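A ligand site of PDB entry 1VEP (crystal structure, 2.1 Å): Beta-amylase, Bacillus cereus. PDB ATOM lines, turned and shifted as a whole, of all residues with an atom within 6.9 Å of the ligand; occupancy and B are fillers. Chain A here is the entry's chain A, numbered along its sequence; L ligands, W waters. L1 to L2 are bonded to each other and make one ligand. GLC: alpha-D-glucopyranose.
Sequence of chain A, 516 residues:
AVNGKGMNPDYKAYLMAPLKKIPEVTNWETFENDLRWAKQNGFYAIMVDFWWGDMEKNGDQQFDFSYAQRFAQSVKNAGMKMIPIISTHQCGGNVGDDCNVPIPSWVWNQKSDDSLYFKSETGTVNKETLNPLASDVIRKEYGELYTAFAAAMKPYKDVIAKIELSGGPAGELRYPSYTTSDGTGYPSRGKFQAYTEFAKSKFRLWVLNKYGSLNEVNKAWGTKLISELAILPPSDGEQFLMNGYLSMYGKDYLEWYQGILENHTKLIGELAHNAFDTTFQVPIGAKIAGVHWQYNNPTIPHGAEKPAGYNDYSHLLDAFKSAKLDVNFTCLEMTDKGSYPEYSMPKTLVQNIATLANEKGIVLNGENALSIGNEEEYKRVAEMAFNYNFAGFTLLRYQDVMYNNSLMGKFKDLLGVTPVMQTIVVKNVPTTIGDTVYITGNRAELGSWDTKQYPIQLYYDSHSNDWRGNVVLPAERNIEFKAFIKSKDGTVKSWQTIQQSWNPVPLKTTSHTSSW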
ATOM      1  N   PHE A 203     -16.192 -30.354  29.735  1.00  0.00           N
ATOM      2  CA  PHE A 203     -16.949 -29.306  29.069  1.00  0.00           C
ATOM      3  C   PHE A 203     -16.930 -28.063  29.960  1.00  0.00           C
ATOM      4  O   PHE A 203     -16.717 -26.949  29.484  1.00  0.00           O
ATOM      5  CB  PHE A 203     -18.400 -29.750  28.827  1.00  0.00           C
ATOM      6  CG  PHE A 203     -19.275 -28.659  28.276  1.00  0.00           C
ATOM      7  CD1 PHE A 203     -18.959 -28.020  27.093  1.00  0.00           C
ATOM      8  CD2 PHE A 203     -20.433 -28.277  28.950  1.00  0.00           C
ATOM      9  CE1 PHE A 203     -19.785 -27.010  26.575  1.00  0.00           C
ATOM     10  CE2 PHE A 203     -21.255 -27.280  28.453  1.00  0.00           C
ATOM     11  CZ  PHE A 203     -20.929 -26.644  27.261  1.00  0.00           C
ATOM     12  N   TRP A 221     -23.561 -16.202  26.927  1.00  0.00           N
ATOM     13  CA  TRP A 221     -24.738 -17.038  26.726  1.00  0.00           C
ATOM     14  C   TRP A 221     -26.041 -16.306  27.022  1.00  0.00           C
ATOM     15  O   TRP A 221     -27.122 -16.807  26.722  1.00  0.00           O
ATOM     16  CB  TRP A 221     -24.667 -18.304  27.598  1.00  0.00           C
ATOM     17  CG  TRP A 221     -23.566 -19.264  27.226  1.00  0.00           C
ATOM     18  CD1 TRP A 221     -22.730 -19.191  26.156  1.00  0.00           C
ATOM     19  CD2 TRP A 221     -23.196 -20.461  27.941  1.00  0.00           C
ATOM     20  NE1 TRP A 221     -21.857 -20.246  26.160  1.00  0.00           N
ATOM     21  CE2 TRP A 221     -22.109 -21.039  27.242  1.00  0.00           C
ATOM     22  CE3 TRP A 221     -23.660 -21.087  29.105  1.00  0.00           C
ATOM     23  CZ2 TRP A 221     -21.497 -22.220  27.675  1.00  0.00           C
ATOM     24  CZ3 TRP A 221     -23.049 -22.257  29.531  1.00  0.00           C
ATOM     25  CH2 TRP A 221     -21.971 -22.813  28.813  1.00  0.00           C
ATOM     26  N   GLY A 222     -25.939 -15.123  27.616  1.00  0.00           N
ATOM     27  CA  GLY A 222     -27.133 -14.387  27.957  1.00  0.00           C
ATOM     28  C   GLY A 222     -27.927 -15.168  28.985  1.00  0.00           C
ATOM     29  O   GLY A 222     -29.160 -15.129  29.008  1.00  0.00           O
ATOM     30  N   THR A 223     -27.218 -15.907  29.836  1.00  0.00           N
ATOM     31  CA  THR A 223     -27.852 -16.715  30.867  1.00  0.00           C
ATOM     32  C   THR A 223     -27.708 -16.127  32.264  1.00  0.00           C
ATOM     33  O   THR A 223     -27.057 -15.104  32.455  1.00  0.00           O
ATOM     34  CB  THR A 223     -27.281 -18.128  30.878  1.00  0.00           C
ATOM     35  OG1 THR A 223     -25.855 -18.076  31.024  1.00  0.00           O
ATOM     36  CG2 THR A 223     -27.630 -18.858  29.595  1.00  0.00           C
ATOM     37  N   LYS A 224     -28.323 -16.796  33.236  1.00  0.00           N
ATOM     38  CA  LYS A 224     -28.280 -16.365  34.629  1.00  0.00           C
ATOM     39  C   LYS A 224     -27.808 -17.504  35.514  1.00  0.00           C
ATOM     40  O   LYS A 224     -28.372 -17.734  36.589  1.00  0.00           O
ATOM     41  CB  LYS A 224     -29.665 -15.901  35.077  1.00  0.00           C
ATOM     42  CG  LYS A 224     -29.716 -14.461  35.551  1.00  0.00           C
ATOM     43  CD  LYS A 224     -29.350 -13.484  34.445  1.00  0.00           C
ATOM     44  CE  LYS A 224     -29.357 -12.052  34.943  1.00  0.00           C
ATOM     45  NZ  LYS A 224     -28.976 -11.091  33.863  1.00  0.00           N
ATOM     46  N   LEU A 225     -26.791 -18.223  35.058  1.00  0.00           N
ATOM     47  CA  LEU A 225     -26.248 -19.339  35.815  1.00  0.00           C
ATOM     48  C   LEU A 225     -25.793 -18.887  37.200  1.00  0.00           C
ATOM     49  O   LEU A 225     -25.038 -17.929  37.346  1.00  0.00           O
ATOM     50  CB  LEU A 225     -25.078 -19.968  35.040  1.00  0.00           C
ATOM     51  CG  LEU A 225     -25.446 -20.912  33.890  1.00  0.00           C
ATOM     52  CD1 LEU A 225     -26.591 -20.362  33.083  1.00  0.00           C
ATOM     53  CD2 LEU A 225     -24.216 -21.118  33.011  1.00  0.00           C
ATOM     54  N   LEU A 229     -21.084 -24.950  38.660  1.00  0.00           N
ATOM     55  CA  LEU A 229     -21.670 -26.282  38.567  1.00  0.00           C
ATOM     56  C   LEU A 229     -22.887 -26.340  37.643  1.00  0.00           C
ATOM     57  O   LEU A 229     -23.306 -27.419  37.239  1.00  0.00           O
ATOM     58  CB  LEU A 229     -22.052 -26.811  39.955  1.00  0.00           C
ATOM     59  CG  LEU A 229     -20.907 -27.213  40.898  1.00  0.00           C
ATOM     60  CD1 LEU A 229     -20.021 -28.238  40.226  1.00  0.00           C
ATOM     61  CD2 LEU A 229     -20.104 -25.980  41.283  1.00  0.00           C
ATOM     62  N   ALA A 230     -23.456 -25.180  37.333  1.00  0.00           N
ATOM     63  CA  ALA A 230     -24.622 -25.115  36.467  1.00  0.00           C
ATOM     64  C   ALA A 230     -24.247 -25.226  34.995  1.00  0.00           C
ATOM     65  O   ALA A 230     -25.100 -25.268  34.110  1.00  0.00           O
ATOM     66  CB  ALA A 230     -25.385 -23.827  36.712  1.00  0.00           C
ATOM     67  N   ILE A 231     -22.941 -25.251  34.730  1.00  0.00           N
ATOM     68  CA  ILE A 231     -22.473 -25.390  33.353  1.00  0.00           C
ATOM     69  C   ILE A 231     -22.510 -26.893  33.106  1.00  0.00           C
ATOM     70  O   ILE A 231     -21.718 -27.643  33.691  1.00  0.00           O
ATOM     71  CB  ILE A 231     -21.022 -24.864  33.201  1.00  0.00           C
ATOM     72  CG1 ILE A 231     -20.989 -23.354  33.464  1.00  0.00           C
ATOM     73  CG2 ILE A 231     -20.512 -25.147  31.798  1.00  0.00           C
ATOM     74  CD1 ILE A 231     -19.614 -22.749  33.424  1.00  0.00           C
ATOM     75  N   LEU A 232     -23.439 -27.324  32.258  1.00  0.00           N
ATOM     76  CA  LEU A 232     -23.604 -28.741  31.958  1.00  0.00           C
ATOM     77  C   LEU A 232     -24.040 -28.951  30.513  1.00  0.00           C
ATOM     78  O   LEU A 232     -24.431 -28.006  29.823  1.00  0.00           O
ATOM     79  CB  LEU A 232     -24.698 -29.331  32.851  1.00  0.00           C
ATOM     80  CG  LEU A 232     -24.606 -29.109  34.356  1.00  0.00           C
ATOM     81  CD1 LEU A 232     -26.015 -29.133  34.929  1.00  0.00           C
ATOM     82  CD2 LEU A 232     -23.718 -30.164  34.993  1.00  0.00           C
ATOM     83  N   PRO A 233     -23.962 -30.199  30.031  1.00  0.00           N
ATOM     84  CA  PRO A 233     -24.378 -30.506  28.657  1.00  0.00           C
ATOM     85  C   PRO A 233     -25.891 -30.357  28.695  1.00  0.00           C
ATOM     86  O   PRO A 233     -26.465 -30.180  29.758  1.00  0.00           O
ATOM     87  CB  PRO A 233     -23.950 -31.970  28.489  1.00  0.00           C
ATOM     88  CG  PRO A 233     -22.844 -32.141  29.491  1.00  0.00           C
ATOM     89  CD  PRO A 233     -23.362 -31.382  30.671  1.00  0.00           C
ATOM     90  N   PRO A 234     -26.566 -30.450  27.539  1.00  0.00           N
ATOM     91  CA  PRO A 234     -28.027 -30.326  27.499  1.00  0.00           C
ATOM     92  C   PRO A 234     -28.768 -31.317  28.396  1.00  0.00           C
ATOM     93  O   PRO A 234     -28.450 -32.508  28.404  1.00  0.00           O
ATOM     94  CB  PRO A 234     -28.355 -30.536  26.028  1.00  0.00           C
ATOM     95  CG  PRO A 234     -27.126 -30.097  25.325  1.00  0.00           C
ATOM     96  CD  PRO A 234     -26.030 -30.681  26.186  1.00  0.00           C
ATOM     97  N   SER A 235     -29.746 -30.826  29.135  1.00  0.00           N
ATOM     98  CA  SER A 235     -30.539 -31.677  30.024  1.00  0.00           C
ATOM     99  C   SER A 235     -31.575 -32.443  29.213  1.00  0.00           C
ATOM    100  O   SER A 235     -31.969 -33.546  29.581  1.00  0.00           O
ATOM    101  CB  SER A 235     -31.257 -30.828  31.081  1.00  0.00           C
ATOM    102  OG  SER A 235     -30.332 -30.242  31.987  1.00  0.00           O
ATOM    103  N   ASP A 236     -32.000 -31.841  28.102  1.00  0.00           N
ATOM    104  CA  ASP A 236     -32.990 -32.445  27.223  1.00  0.00           C
ATOM    105  C   ASP A 236     -32.447 -32.388  25.792  1.00  0.00           C
ATOM    106  O   ASP A 236     -32.497 -31.344  25.141  1.00  0.00           O
ATOM    107  CB  ASP A 236     -34.297 -31.658  27.294  1.00  0.00           C
ATOM    108  CG  ASP A 236     -35.399 -32.267  26.449  1.00  0.00           C
ATOM    109  OD1 ASP A 236     -35.089 -32.849  25.387  1.00  0.00           O
ATOM    110  OD2 ASP A 236     -36.569 -32.152  26.847  1.00  0.00           O
ATOM    111  N   GLY A 237     -31.947 -33.517  25.306  1.00  0.00           N
ATOM    112  CA  GLY A 237     -31.400 -33.559  23.962  1.00  0.00           C
ATOM    113  C   GLY A 237     -32.377 -33.207  22.863  1.00  0.00           C
ATOM    114  O   GLY A 237     -32.005 -32.636  21.848  1.00  0.00           O
ATOM    115  N   GLN A 239     -35.092 -31.133  23.079  1.00  0.00           N
ATOM    116  CA  GLN A 239     -35.351 -29.701  23.063  1.00  0.00           C
ATOM    117  C   GLN A 239     -34.106 -29.011  22.507  1.00  0.00           C
ATOM    118  O   GLN A 239     -34.216 -28.038  21.745  1.00  0.00           O
ATOM    119  CB  GLN A 239     -35.668 -29.216  24.491  1.00  0.00           C
ATOM    120  CG  GLN A 239     -35.790 -27.706  24.614  1.00  0.00           C
ATOM    121  CD  GLN A 239     -34.467 -27.040  24.932  1.00  0.00           C
ATOM    122  OE1 GLN A 239     -34.268 -25.859  24.639  1.00  0.00           O
ATOM    123  NE2 GLN A 239     -33.550 -27.785  25.547  1.00  0.00           N
ATOM    124  N   PHE A 240     -32.935 -29.528  22.850  1.00  0.00           N
ATOM    125  CA  PHE A 240     -31.689 -28.948  22.346  1.00  0.00           C
ATOM    126  C   PHE A 240     -31.623 -29.041  20.824  1.00  0.00           C
ATOM    127  O   PHE A 240     -31.202 -28.095  20.166  1.00  0.00           O
ATOM    128  CB  PHE A 240     -30.469 -29.664  22.929  1.00  0.00           C
ATOM    129  CG  PHE A 240     -29.166 -29.071  22.469  1.00  0.00           C
ATOM    130  CD1 PHE A 240     -28.632 -27.946  23.098  1.00  0.00           C
ATOM    131  CD2 PHE A 240     -28.495 -29.617  21.377  1.00  0.00           C
ATOM    132  CE1 PHE A 240     -27.445 -27.369  22.636  1.00  0.00           C
ATOM    133  CE2 PHE A 240     -27.309 -29.038  20.900  1.00  0.00           C
ATOM    134  CZ  PHE A 240     -26.782 -27.906  21.530  1.00  0.00           C
ATOM    135  N   LEU A 241     -32.043 -30.176  20.275  1.00  0.00           N
ATOM    136  CA  LEU A 241     -32.019 -30.390  18.822  1.00  0.00           C
ATOM    137  C   LEU A 241     -33.177 -29.671  18.118  1.00  0.00           C
ATOM    138  O   LEU A 241     -33.134 -29.441  16.914  1.00  0.00           O
ATOM    139  CB  LEU A 241     -32.071 -31.894  18.497  1.00  0.00           C
ATOM    140  CG  LEU A 241     -30.896 -32.780  18.927  1.00  0.00           C
ATOM    141  CD1 LEU A 241     -31.284 -34.251  18.748  1.00  0.00           C
ATOM    142  CD2 LEU A 241     -29.662 -32.471  18.089  1.00  0.00           C
ATOM    143  N   ASN A 243     -34.387 -26.482  19.062  1.00  0.00           N
ATOM    144  CA  ASN A 243     -34.038 -25.070  18.893  1.00  0.00           C
ATOM    145  C   ASN A 243     -32.924 -24.562  19.789  1.00  0.00           C
ATOM    146  O   ASN A 243     -32.397 -23.476  19.561  1.00  0.00           O
ATOM    147  CB  ASN A 243     -35.279 -24.190  19.041  1.00  0.00           C
ATOM    148  CG  ASN A 243     -36.112 -24.537  20.246  1.00  0.00           C
ATOM    149  OD1 ASN A 243     -37.336 -24.516  20.182  1.00  0.00           O
ATOM    150  ND2 ASN A 243     -35.450 -24.848  21.361  1.00  0.00           N
ATOM    151  N   GLY A 244     -32.556 -25.338  20.804  1.00  0.00           N
ATOM    152  CA  GLY A 244     -31.484 -24.914  21.685  1.00  0.00           C
ATOM    153  C   GLY A 244     -30.150 -24.786  20.955  1.00  0.00           C
ATOM    154  O   GLY A 244     -29.290 -23.983  21.338  1.00  0.00           O
ATOM    155  N   TYR A 245     -29.966 -25.572  19.895  1.00  0.00           N
ATOM    156  CA  TYR A 245     -28.715 -25.522  19.156  1.00  0.00           C
ATOM    157  C   TYR A 245     -28.486 -24.157  18.541  1.00  0.00           C
ATOM    158  O   TYR A 245     -27.357 -23.800  18.223  1.00  0.00           O
ATOM    159  CB  TYR A 245     -28.701 -26.564  18.037  1.00  0.00           C
ATOM    160  CG  TYR A 245     -29.716 -26.310  16.958  1.00  0.00           C
ATOM    161  CD1 TYR A 245     -31.061 -26.579  17.169  1.00  0.00           C
ATOM    162  CD2 TYR A 245     -29.328 -25.799  15.724  1.00  0.00           C
ATOM    163  CE1 TYR A 245     -31.996 -26.362  16.171  1.00  0.00           C
ATOM    164  CE2 TYR A 245     -30.253 -25.572  14.712  1.00  0.00           C
ATOM    165  CZ  TYR A 245     -31.595 -25.854  14.944  1.00  0.00           C
ATOM    166  OH  TYR A 245     -32.511 -25.672  13.935  1.00  0.00           O
ATOM    167  N   SER A 247     -28.936 -21.201  19.981  1.00  0.00           N
ATOM    168  CA  SER A 247     -28.405 -20.227  20.930  1.00  0.00           C
ATOM    169  C   SER A 247     -26.875 -20.221  20.991  1.00  0.00           C
ATOM    170  O   SER A 247     -26.214 -21.094  20.423  1.00  0.00           O
ATOM    171  CB  SER A 247     -28.941 -20.520  22.334  1.00  0.00           C
ATOM    172  OG  SER A 247     -28.356 -21.719  22.832  1.00  0.00           O
ATOM    173  N   TYR A 249     -25.151 -20.766  23.580  1.00  0.00           N
ATOM    174  CA  TYR A 249     -24.768 -21.903  24.396  1.00  0.00           C
ATOM    175  C   TYR A 249     -24.660 -23.102  23.465  1.00  0.00           C
ATOM    176  O   TYR A 249     -23.679 -23.827  23.482  1.00  0.00           O
ATOM    177  CB  TYR A 249     -25.823 -22.190  25.471  1.00  0.00           C
ATOM    178  CG  TYR A 249     -25.745 -23.612  26.028  1.00  0.00           C
ATOM    179  CD1 TYR A 249     -24.705 -23.994  26.877  1.00  0.00           C
ATOM    180  CD2 TYR A 249     -26.686 -24.584  25.658  1.00  0.00           C
ATOM    181  CE1 TYR A 249     -24.599 -25.302  27.336  1.00  0.00           C
ATOM    182  CE2 TYR A 249     -26.580 -25.904  26.110  1.00  0.00           C
ATOM    183  CZ  TYR A 249     -25.531 -26.253  26.960  1.00  0.00           C
ATOM    184  OH  TYR A 249     -25.411 -27.546  27.397  1.00  0.00           O
ATOM    185  N   GLY A 250     -25.695 -23.275  22.650  1.00  0.00           N
ATOM    186  CA  GLY A 250     -25.738 -24.389  21.718  1.00  0.00           C
ATOM    187  C   GLY A 250     -24.510 -24.456  20.847  1.00  0.00           C
ATOM    188  O   GLY A 250     -23.859 -25.504  20.741  1.00  0.00           O
HETATM  189  C1  GLC L   1     -30.930 -24.009  25.449  1.00  0.00           C
HETATM  190  C2  GLC L   1     -30.535 -25.495  25.340  1.00  0.00           C
HETATM  191  C3  GLC L   1     -30.393 -26.107  26.738  1.00  0.00           C
HETATM  192  C4  GLC L   1     -29.466 -25.257  27.615  1.00  0.00           C
HETATM  193  C5  GLC L   1     -29.934 -23.801  27.616  1.00  0.00           C
HETATM  194  C6  GLC L   1     -28.988 -22.894  28.380  1.00  0.00           C
HETATM  195  O1  GLC L   1     -32.180 -23.905  26.018  1.00  0.00           O
HETATM  196  O2  GLC L   1     -31.521 -26.194  24.605  1.00  0.00           O
HETATM  197  O3  GLC L   1     -29.865 -27.409  26.631  1.00  0.00           O
HETATM  198  O4  GLC L   1     -29.464 -25.768  28.962  1.00  0.00           O
HETATM  199  O5  GLC L   1     -29.989 -23.293  26.260  1.00  0.00           O
HETATM  200  O6  GLC L   1     -29.532 -21.601  28.552  1.00  0.00           O
HETATM  201  C1  GLC L   2     -28.339 -26.535  29.275  1.00  0.00           C
HETATM  202  C2  GLC L   2     -28.665 -27.524  30.412  1.00  0.00           C
HETATM  203  C3  GLC L   2     -28.708 -26.809  31.772  1.00  0.00           C
HETATM  204  C4  GLC L   2     -27.447 -25.985  31.992  1.00  0.00           C
HETATM  205  C5  GLC L   2     -27.263 -25.015  30.820  1.00  0.00           C
HETATM  206  C6  GLC L   2     -25.978 -24.220  30.929  1.00  0.00           C
HETATM  207  O2  GLC L   2     -29.920 -28.133  30.160  1.00  0.00           O
HETATM  208  O3  GLC L   2     -28.844 -27.773  32.804  1.00  0.00           O
HETATM  209  O4  GLC L   2     -27.527 -25.269  33.222  1.00  0.00           O
HETATM  210  O5  GLC L   2     -27.190 -25.747  29.576  1.00  0.00           O
HETATM  211  O6  GLC L   2     -24.863 -25.097  30.959  1.00  0.00           O
HETATM  212  O   HOH W   1     -30.336 -21.729  31.653  1.00  0.00           O
HETATM  213  O   HOH W   2     -32.553 -27.361  30.119  1.00  0.00           O
HETATM  214  O   HOH W   3     -31.856 -29.118  26.978  1.00  0.00           O
HETATM  215  O   HOH W   4     -29.409 -20.114  25.754  1.00  0.00           O
HETATM  216  O   HOH W   5     -29.851 -23.316  33.595  1.00  0.00           O
HETATM  217  O   HOH W   6     -32.697 -21.732  23.584  1.00  0.00           O
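Trp 221 touches the ligand. CG2 of Thr 223 touches O6 of GLC L1, at 3.5 Å. Ile 231 touches the ligand. O of Pro 233 touches C2 of GLC L2, at 3.5 Å. Pro 234 touches the ligand. Phe 240 touches the ligand. Gly 244 touches the ligand. Hydrophobic or aromatic side chains that line the ligand: Trp 221, Leu 232, Pro 234, Phe 240 and Tyr 249. Within 4 Å of the ligand: Trp 221, Thr 223, Ala 230, Ile 231, Leu 232, Pro 233, Pro 234, Ser 235, Gln 239, Phe 240, Gly 244 and Tyr 249. The nearest printed residue that does not touch the ligand is Ser 247 (4.1 Å).
O of Ala 230 is in hydrogen-bond range of O4 of GLC L2 (2.6 Å). NE2 of Gln 239 sits at hydrogen-bond distance from O2 of GLC L1, 2.7 Å away. N of Ser 235 lies within hydrogen-bond range of O2 of GLC L2, 2.9 Å away. O2 of GLC L2 is in hydrogen-bond range of OG of Ser 235, at 2.8 Å. N of Leu 232 lies within hydrogen-bond range of O6 of GLC L2, 2.9 Å away. O of Leu 232 sits at hydrogen-bond distance from O6 of GLC L2. An oxygen (O5) of GLC L2 lies close to the side-chain hydroxyl (OH) of Tyr 249 (3.3 Å).
Water W4 lies within hydrogen-bond range of O6 of GLC L1 and OG of Ser 247.
The backbone NH of Gly 244 lies within hydrogen-bond range of the backbone carbonyl oxygen of Gln 239 (3.3 Å). The backbone NH (N) of Gln 239 sits at hydrogen-bond distance from the side-chain carboxylate (OD1) of Asp 236, 2.9 Å away. The backbone carbonyl oxygen of Gln 239 sits at hydrogen-bond distance from the side-chain amide nitrogen of Asn 243 (3.4 Å). The backbone carbonyl oxygen (O) of Leu 232 lies within hydrogen-bond range of the side-chain hydroxyl (OH) of Tyr 249, 2.7 Å away. N of Tyr 249 sits close to OG of Ser 247, at 3.4 Å. O of Gly 244 lies within hydrogen-bond range of OG of Ser 247. The backbone carbonyl oxygen (O) of Phe 240 is in hydrogen-bond range of the backbone NH (N) of Tyr 245.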
